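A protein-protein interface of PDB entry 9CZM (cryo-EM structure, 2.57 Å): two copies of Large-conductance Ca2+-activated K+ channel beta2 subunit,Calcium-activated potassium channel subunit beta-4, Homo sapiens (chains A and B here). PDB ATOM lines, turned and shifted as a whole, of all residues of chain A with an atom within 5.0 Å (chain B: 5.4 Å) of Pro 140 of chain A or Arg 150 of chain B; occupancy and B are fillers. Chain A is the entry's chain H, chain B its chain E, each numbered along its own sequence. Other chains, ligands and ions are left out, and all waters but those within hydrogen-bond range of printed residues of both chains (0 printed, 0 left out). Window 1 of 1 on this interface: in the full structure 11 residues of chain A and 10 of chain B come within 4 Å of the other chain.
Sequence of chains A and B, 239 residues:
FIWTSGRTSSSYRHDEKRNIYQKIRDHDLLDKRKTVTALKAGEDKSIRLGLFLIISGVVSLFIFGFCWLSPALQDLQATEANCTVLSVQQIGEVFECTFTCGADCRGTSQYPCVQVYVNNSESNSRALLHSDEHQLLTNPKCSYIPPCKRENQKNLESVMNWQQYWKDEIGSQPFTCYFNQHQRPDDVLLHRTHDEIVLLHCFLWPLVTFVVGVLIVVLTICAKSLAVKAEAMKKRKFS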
ATOM      1  N   LEU A 128      16.547  32.597  -4.136  1.00  0.00           N
ATOM      2  CA  LEU A 128      16.846  32.258  -5.528  1.00  0.00           C
ATOM      3  C   LEU A 128      16.743  33.497  -6.425  1.00  0.00           C
ATOM      4  O   LEU A 128      15.714  34.165  -6.463  1.00  0.00           O
ATOM      5  CB  LEU A 128      15.907  31.119  -5.955  1.00  0.00           C
ATOM      6  CG  LEU A 128      15.964  30.700  -7.435  1.00  0.00           C
ATOM      7  CD1 LEU A 128      17.368  30.381  -7.935  1.00  0.00           C
ATOM      8  CD2 LEU A 128      15.130  29.433  -7.615  1.00  0.00           C
ATOM      9  N   HIS A 130      16.184  35.223  -9.979  1.00  0.00           N
ATOM     10  CA  HIS A 130      15.487  34.942 -11.223  1.00  0.00           C
ATOM     11  C   HIS A 130      15.716  35.955 -12.407  1.00  0.00           C
ATOM     12  O   HIS A 130      15.048  35.869 -13.434  1.00  0.00           O
ATOM     13  CB  HIS A 130      14.012  34.966 -10.830  1.00  0.00           C
ATOM     14  CG  HIS A 130      13.601  33.825  -9.954  1.00  0.00           C
ATOM     15  ND1 HIS A 130      13.382  33.971  -8.601  1.00  0.00           N
ATOM     16  CD2 HIS A 130      13.374  32.519 -10.235  1.00  0.00           C
ATOM     17  CE1 HIS A 130      13.036  32.804  -8.086  1.00  0.00           C
ATOM     18  NE2 HIS A 130      13.024  31.908  -9.056  1.00  0.00           N
ATOM     19  N   GLN A 135      10.858  35.634 -16.301  1.00  0.00           N
ATOM     20  CA  GLN A 135      11.551  34.370 -16.042  1.00  0.00           C
ATOM     21  C   GLN A 135      10.927  33.646 -14.848  1.00  0.00           C
ATOM     22  O   GLN A 135      10.580  32.468 -14.928  1.00  0.00           O
ATOM     23  CB  GLN A 135      13.041  34.629 -15.802  1.00  0.00           C
ATOM     24  CG  GLN A 135      13.893  33.375 -15.821  1.00  0.00           C
ATOM     25  CD  GLN A 135      13.861  32.628 -14.504  1.00  0.00           C
ATOM     26  OE1 GLN A 135      13.592  33.208 -13.453  1.00  0.00           O
ATOM     27  NE2 GLN A 135      14.134  31.330 -14.554  1.00  0.00           N
ATOM     28  N   LEU A 136      10.789  34.371 -13.744  1.00  0.00           N
ATOM     29  CA  LEU A 136      10.154  33.836 -12.539  1.00  0.00           C
ATOM     30  C   LEU A 136       8.764  33.281 -12.863  1.00  0.00           C
ATOM     31  O   LEU A 136       8.450  32.145 -12.520  1.00  0.00           O
ATOM     32  CB  LEU A 136      10.112  34.952 -11.479  1.00  0.00           C
ATOM     33  CG  LEU A 136       9.687  34.543 -10.056  1.00  0.00           C
ATOM     34  CD1 LEU A 136       9.999  35.706  -9.114  1.00  0.00           C
ATOM     35  CD2 LEU A 136       8.191  34.259  -9.895  1.00  0.00           C
ATOM     36  N   THR A 138       7.515  32.221 -15.723  1.00  0.00           N
ATOM     37  CA  THR A 138       7.550  31.098 -16.677  1.00  0.00           C
ATOM     38  C   THR A 138       8.251  29.846 -16.145  1.00  0.00           C
ATOM     39  O   THR A 138       7.788  28.745 -16.447  1.00  0.00           O
ATOM     40  CB  THR A 138       8.167  31.513 -18.018  1.00  0.00           C
ATOM     41  OG1 THR A 138       9.386  32.188 -17.843  1.00  0.00           O
ATOM     42  CG2 THR A 138       7.243  32.434 -18.802  1.00  0.00           C
ATOM     43  N   ASN A 139       9.312  29.963 -15.340  1.00  0.00           N
ATOM     44  CA  ASN A 139       9.969  28.823 -14.689  1.00  0.00           C
ATOM     45  C   ASN A 139      10.788  29.245 -13.445  1.00  0.00           C
ATOM     46  O   ASN A 139      11.989  29.511 -13.552  1.00  0.00           O
ATOM     47  CB  ASN A 139      10.862  28.093 -15.709  1.00  0.00           C
ATOM     48  CG  ASN A 139      11.492  26.841 -15.128  1.00  0.00           C
ATOM     49  OD1 ASN A 139      11.333  26.498 -13.965  1.00  0.00           O
ATOM     50  ND2 ASN A 139      12.216  26.112 -15.937  1.00  0.00           N
ATOM     51  N   PRO A 140      10.189  29.254 -12.241  1.00  0.00           N
ATOM     52  CA  PRO A 140      10.844  29.744 -11.034  1.00  0.00           C
ATOM     53  C   PRO A 140      11.867  28.770 -10.430  1.00  0.00           C
ATOM     54  O   PRO A 140      12.537  29.141  -9.468  1.00  0.00           O
ATOM     55  CB  PRO A 140       9.704  30.045 -10.061  1.00  0.00           C
ATOM     56  CG  PRO A 140       8.661  29.006 -10.444  1.00  0.00           C
ATOM     57  CD  PRO A 140       8.824  28.864 -11.953  1.00  0.00           C
ATOM     58  N   LYS A 141      11.951  27.538 -10.932  1.00  0.00           N
ATOM     59  CA  LYS A 141      12.967  26.571 -10.463  1.00  0.00           C
ATOM     60  C   LYS A 141      14.421  26.814 -10.996  1.00  0.00           C
ATOM     61  O   LYS A 141      15.383  26.287 -10.440  1.00  0.00           O
ATOM     62  CB  LYS A 141      12.514  25.145 -10.780  1.00  0.00           C
ATOM     63  CG  LYS A 141      11.230  24.754 -10.063  1.00  0.00           C
ATOM     64  CD  LYS A 141      11.059  23.247  -9.992  1.00  0.00           C
ATOM     65  CE  LYS A 141      11.766  22.650  -8.787  1.00  0.00           C
ATOM     66  NZ  LYS A 141      11.935  21.181  -8.950  1.00  0.00           N
ATOM     67  N   CYS A 142      14.549  27.603 -12.064  1.00  0.00           N
ATOM     68  CA  CYS A 142      15.821  27.996 -12.665  1.00  0.00           C
ATOM     69  C   CYS A 142      16.014  29.511 -12.517  1.00  0.00           C
ATOM     70  O   CYS A 142      15.051  30.260 -12.406  1.00  0.00           O
ATOM     71  CB  CYS A 142      15.876  27.553 -14.133  1.00  0.00           C
ATOM     72  SG  CYS A 142      15.253  25.882 -14.450  1.00  0.00           S
ATOM     73  N   ASP A 186      11.713  34.297  -0.893  1.00  0.00           N
ATOM     74  CA  ASP A 186      12.754  33.412  -1.419  1.00  0.00           C
ATOM     75  C   ASP A 186      13.015  33.586  -2.935  1.00  0.00           C
ATOM     76  O   ASP A 186      13.737  32.775  -3.517  1.00  0.00           O
ATOM     77  CB  ASP A 186      12.441  31.957  -1.021  1.00  0.00           C
ATOM     78  CG  ASP A 186      11.026  31.450  -1.351  1.00  0.00           C
ATOM     79  OD1 ASP A 186      10.182  32.211  -1.870  1.00  0.00           O
ATOM     80  OD2 ASP A 186      10.753  30.270  -1.034  1.00  0.00           O
ATOM     81  N   ASP A 187      12.512  34.665  -3.550  1.00  0.00           N
ATOM     82  CA  ASP A 187      12.779  35.044  -4.950  1.00  0.00           C
ATOM     83  C   ASP A 187      13.422  36.438  -5.037  1.00  0.00           C
ATOM     84  O   ASP A 187      13.026  37.344  -4.308  1.00  0.00           O
ATOM     85  CB  ASP A 187      11.486  35.069  -5.782  1.00  0.00           C
ATOM     86  CG  ASP A 187      10.621  33.808  -5.680  1.00  0.00           C
ATOM     87  OD1 ASP A 187      11.181  32.694  -5.627  1.00  0.00           O
ATOM     88  OD2 ASP A 187       9.373  33.912  -5.712  1.00  0.00           O
ATOM     89  N   PHE B  99       3.751  23.298  -6.359  1.00  0.00           N
ATOM     90  CA  PHE B  99       3.874  24.345  -5.339  1.00  0.00           C
ATOM     91  C   PHE B  99       3.320  25.677  -5.851  1.00  0.00           C
ATOM     92  O   PHE B  99       3.305  25.947  -7.041  1.00  0.00           O
ATOM     93  CB  PHE B  99       5.321  24.466  -4.825  1.00  0.00           C
ATOM     94  CG  PHE B  99       6.347  25.084  -5.758  1.00  0.00           C
ATOM     95  CD1 PHE B  99       6.414  26.478  -5.931  1.00  0.00           C
ATOM     96  CD2 PHE B  99       7.283  24.267  -6.410  1.00  0.00           C
ATOM     97  CE1 PHE B  99       7.380  27.042  -6.784  1.00  0.00           C
ATOM     98  CE2 PHE B  99       8.262  24.831  -7.244  1.00  0.00           C
ATOM     99  CZ  PHE B  99       8.306  26.219  -7.439  1.00  0.00           C
ATOM    100  N   CYS B 101       4.019  29.914  -5.096  1.00  0.00           N
ATOM    101  CA  CYS B 101       4.742  31.004  -4.455  1.00  0.00           C
ATOM    102  C   CYS B 101       3.808  31.988  -3.723  1.00  0.00           C
ATOM    103  O   CYS B 101       4.275  32.833  -2.963  1.00  0.00           O
ATOM    104  CB  CYS B 101       5.480  31.794  -5.538  1.00  0.00           C
ATOM    105  SG  CYS B 101       6.293  30.898  -6.884  1.00  0.00           S
ATOM    106  N   CYS B 105       2.018  30.923  -9.703  1.00  0.00           N
ATOM    107  CA  CYS B 105       3.091  29.929  -9.857  1.00  0.00           C
ATOM    108  C   CYS B 105       2.553  28.504 -10.111  1.00  0.00           C
ATOM    109  O   CYS B 105       1.486  28.143  -9.626  1.00  0.00           O
ATOM    110  CB  CYS B 105       3.981  29.940  -8.610  1.00  0.00           C
ATOM    111  SG  CYS B 105       5.138  31.320  -8.510  1.00  0.00           S
ATOM    112  N   GLY B 107       5.229  25.467 -10.589  1.00  0.00           N
ATOM    113  CA  GLY B 107       6.235  24.796  -9.785  1.00  0.00           C
ATOM    114  C   GLY B 107       6.209  23.266  -9.767  1.00  0.00           C
ATOM    115  O   GLY B 107       6.526  22.668  -8.754  1.00  0.00           O
ATOM    116  N   SER B 109       6.791  19.613  -9.327  1.00  0.00           N
ATOM    117  CA  SER B 109       7.948  19.024  -8.640  1.00  0.00           C
ATOM    118  C   SER B 109       7.672  17.607  -8.136  1.00  0.00           C
ATOM    119  O   SER B 109       6.608  17.322  -7.592  1.00  0.00           O
ATOM    120  CB  SER B 109       8.374  19.915  -7.468  1.00  0.00           C
ATOM    121  OG  SER B 109       8.775  21.185  -7.945  1.00  0.00           O
ATOM    122  N   CYS B 148       3.485  20.579  -0.842  1.00  0.00           N
ATOM    123  CA  CYS B 148       4.371  20.750  -1.993  1.00  0.00           C
ATOM    124  C   CYS B 148       5.218  22.032  -1.893  1.00  0.00           C
ATOM    125  O   CYS B 148       4.723  23.078  -1.462  1.00  0.00           O
ATOM    126  CB  CYS B 148       3.560  20.717  -3.286  1.00  0.00           C
ATOM    127  SG  CYS B 148       4.571  20.415  -4.755  1.00  0.00           S
ATOM    128  N   LYS B 149       6.496  21.959  -2.282  1.00  0.00           N
ATOM    129  CA  LYS B 149       7.498  23.002  -2.018  1.00  0.00           C
ATOM    130  C   LYS B 149       8.427  23.239  -3.215  1.00  0.00           C
ATOM    131  O   LYS B 149       8.563  22.382  -4.082  1.00  0.00           O
ATOM    132  CB  LYS B 149       8.272  22.596  -0.742  1.00  0.00           C
ATOM    133  CG  LYS B 149       8.998  23.729   0.005  1.00  0.00           C
ATOM    134  CD  LYS B 149       8.106  24.905   0.444  1.00  0.00           C
ATOM    135  CE  LYS B 149       6.891  24.450   1.264  1.00  0.00           C
ATOM    136  NZ  LYS B 149       6.081  25.605   1.723  1.00  0.00           N
ATOM    137  N   ARG B 150       9.102  24.384  -3.258  1.00  0.00           N
ATOM    138  CA  ARG B 150       9.994  24.703  -4.385  1.00  0.00           C
ATOM    139  C   ARG B 150      11.233  23.802  -4.543  1.00  0.00           C
ATOM    140  O   ARG B 150      11.854  23.767  -5.604  1.00  0.00           O
ATOM    141  CB  ARG B 150      10.425  26.170  -4.316  1.00  0.00           C
ATOM    142  CG  ARG B 150      11.782  26.447  -4.945  1.00  0.00           C
ATOM    143  CD  ARG B 150      11.649  27.339  -6.167  1.00  0.00           C
ATOM    144  NE  ARG B 150      10.549  28.289  -6.033  1.00  0.00           N
ATOM    145  CZ  ARG B 150      10.702  29.569  -5.707  1.00  0.00           C
ATOM    146  NH1 ARG B 150       9.643  30.360  -5.608  1.00  0.00           N
ATOM    147  NH2 ARG B 150      11.913  30.057  -5.481  1.00  0.00           N
ATOM    148  N   GLU B 151      11.577  23.084  -3.482  1.00  0.00           N
ATOM    149  CA  GLU B 151      12.736  22.184  -3.426  1.00  0.00           C
ATOM    150  C   GLU B 151      12.339  20.701  -3.376  1.00  0.00           C
ATOM    151  O   GLU B 151      11.683  20.257  -2.429  1.00  0.00           O
ATOM    152  CB  GLU B 151      13.555  22.521  -2.166  1.00  0.00           C
ATOM    153  CG  GLU B 151      14.543  23.674  -2.368  1.00  0.00           C
ATOM    154  CD  GLU B 151      15.869  23.182  -2.964  1.00  0.00           C
ATOM    155  OE1 GLU B 151      15.848  22.306  -3.856  1.00  0.00           O
ATOM    156  OE2 GLU B 151      16.936  23.653  -2.515  1.00  0.00           O
ATOM    157  N   ASN B 152      12.843  19.901  -4.324  1.00  0.00           N
ATOM    158  CA  ASN B 152      12.670  18.445  -4.331  1.00  0.00           C
ATOM    159  C   ASN B 152      13.188  17.811  -3.029  1.00  0.00           C
ATOM    160  O   ASN B 152      12.538  16.934  -2.468  1.00  0.00           O
ATOM    161  CB  ASN B 152      13.418  17.833  -5.531  1.00  0.00           C
ATOM    162  CG  ASN B 152      12.816  18.164  -6.885  1.00  0.00           C
ATOM    163  OD1 ASN B 152      12.757  19.311  -7.305  1.00  0.00           O
ATOM    164  ND2 ASN B 152      12.382  17.168  -7.619  1.00  0.00           N
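The side-chain hydroxyl (OG) of Ser 109 of chain B is in hydrogen-bond range of the side-chain amino group (NZ) of Lys 141 of chain A, 3.3 Å away. The side-chain amino group (NZ) of Lys 141 of chain A lies within hydrogen-bond range of the side-chain amide oxygen (OD1) of Asn 152 of chain B. OD1 of Asp 187 of chain A is in salt-bridge range of NH2 of Arg 150 of chain B.
The backbone carbonyl oxygen (O) of Gly 107 of chain B is in hydrogen-bond range of the side-chain hydroxyl (OG) of Ser 109 of chain B (2.8 Å). The side-chain sulfur (SG) of Cys 101 of chain B is in hydrogen-bond range of the guanidinium group (NH1) of Arg 150 of chain B (3.6 Å). A ring nitrogen (ND1) of His 130 of chain A is in hydrogen-bond range of the backbone carbonyl oxygen (O) of Leu 128 of chain A, at 3.2 Å. A ring nitrogen (NE2) of His 130 of chain A sits at hydrogen-bond distance from the backbone carbonyl oxygen of Pro 140 of chain A (2.8 Å). The side-chain sulfur of Cys 105 of chain B is disulfide-bonded to the side-chain sulfur of Cys 101 of chain B, 2.0 Å away. OE1 of Gln 135 of chain A lies close to O of His 130 of chain A (3.0 Å).
Among the printed residues, merely in contact across the chains: Leu 128 of chain A with Arg 150 of chain B (3.9 Å), His 130 of chain A with Arg 150 of chain B (3.9 Å), Pro 140 of chain A with Arg 150 of chain B (3.9 Å), Lys 141 of chain A with Arg 150 of chain B (3.4 Å) and Asp 186 of chain A with Arg 150 of chain B (3.8 Å).
Of the printed residues of chain B, Leu 128 of chain A touches Arg 150 (3.9 Å). Of chain B, only Arg 150 comes within 4 Å of Pro 140 of chain A. Of the printed residues of chain B, Lys 141 of chain A touches Ser 109 (3.3 Å), Arg 150 (3.4 Å) and Asn 152 (2.6 Å). Printed residues of chain B within 4 Å of Asp 186 of chain A: Arg 150. Of the printed residues of chain B, Asp 187 of chain A touches Arg 150. Arg 150 of chain B touches just these residues of chain A: Leu 128, His 130, Pro 140, Lys 141, Asp 186 and Asp 187. Of the printed residues of chain A, Asn 152 of chain B touches Lys 141 (2.6 Å).
Printed residues of chain B that touch a printed residue of chain A: Ser 109, Arg 150 and Asn 152. Hydrophobic or aromatic side chains of chain A within 4 Å of the printed part of chain B: Leu 128 and His 130. Among the printed residues, Asp or Glu carboxylates within 4 Å of a Lys or Arg side-chain nitrogen of the other chain: Asp 187 of chain A with Arg 150 of chain B.
No position is printed for both chains. Of the 8 pairs that touch across the chains among the printed residues, none has its exchanged pair printed and touching as well.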
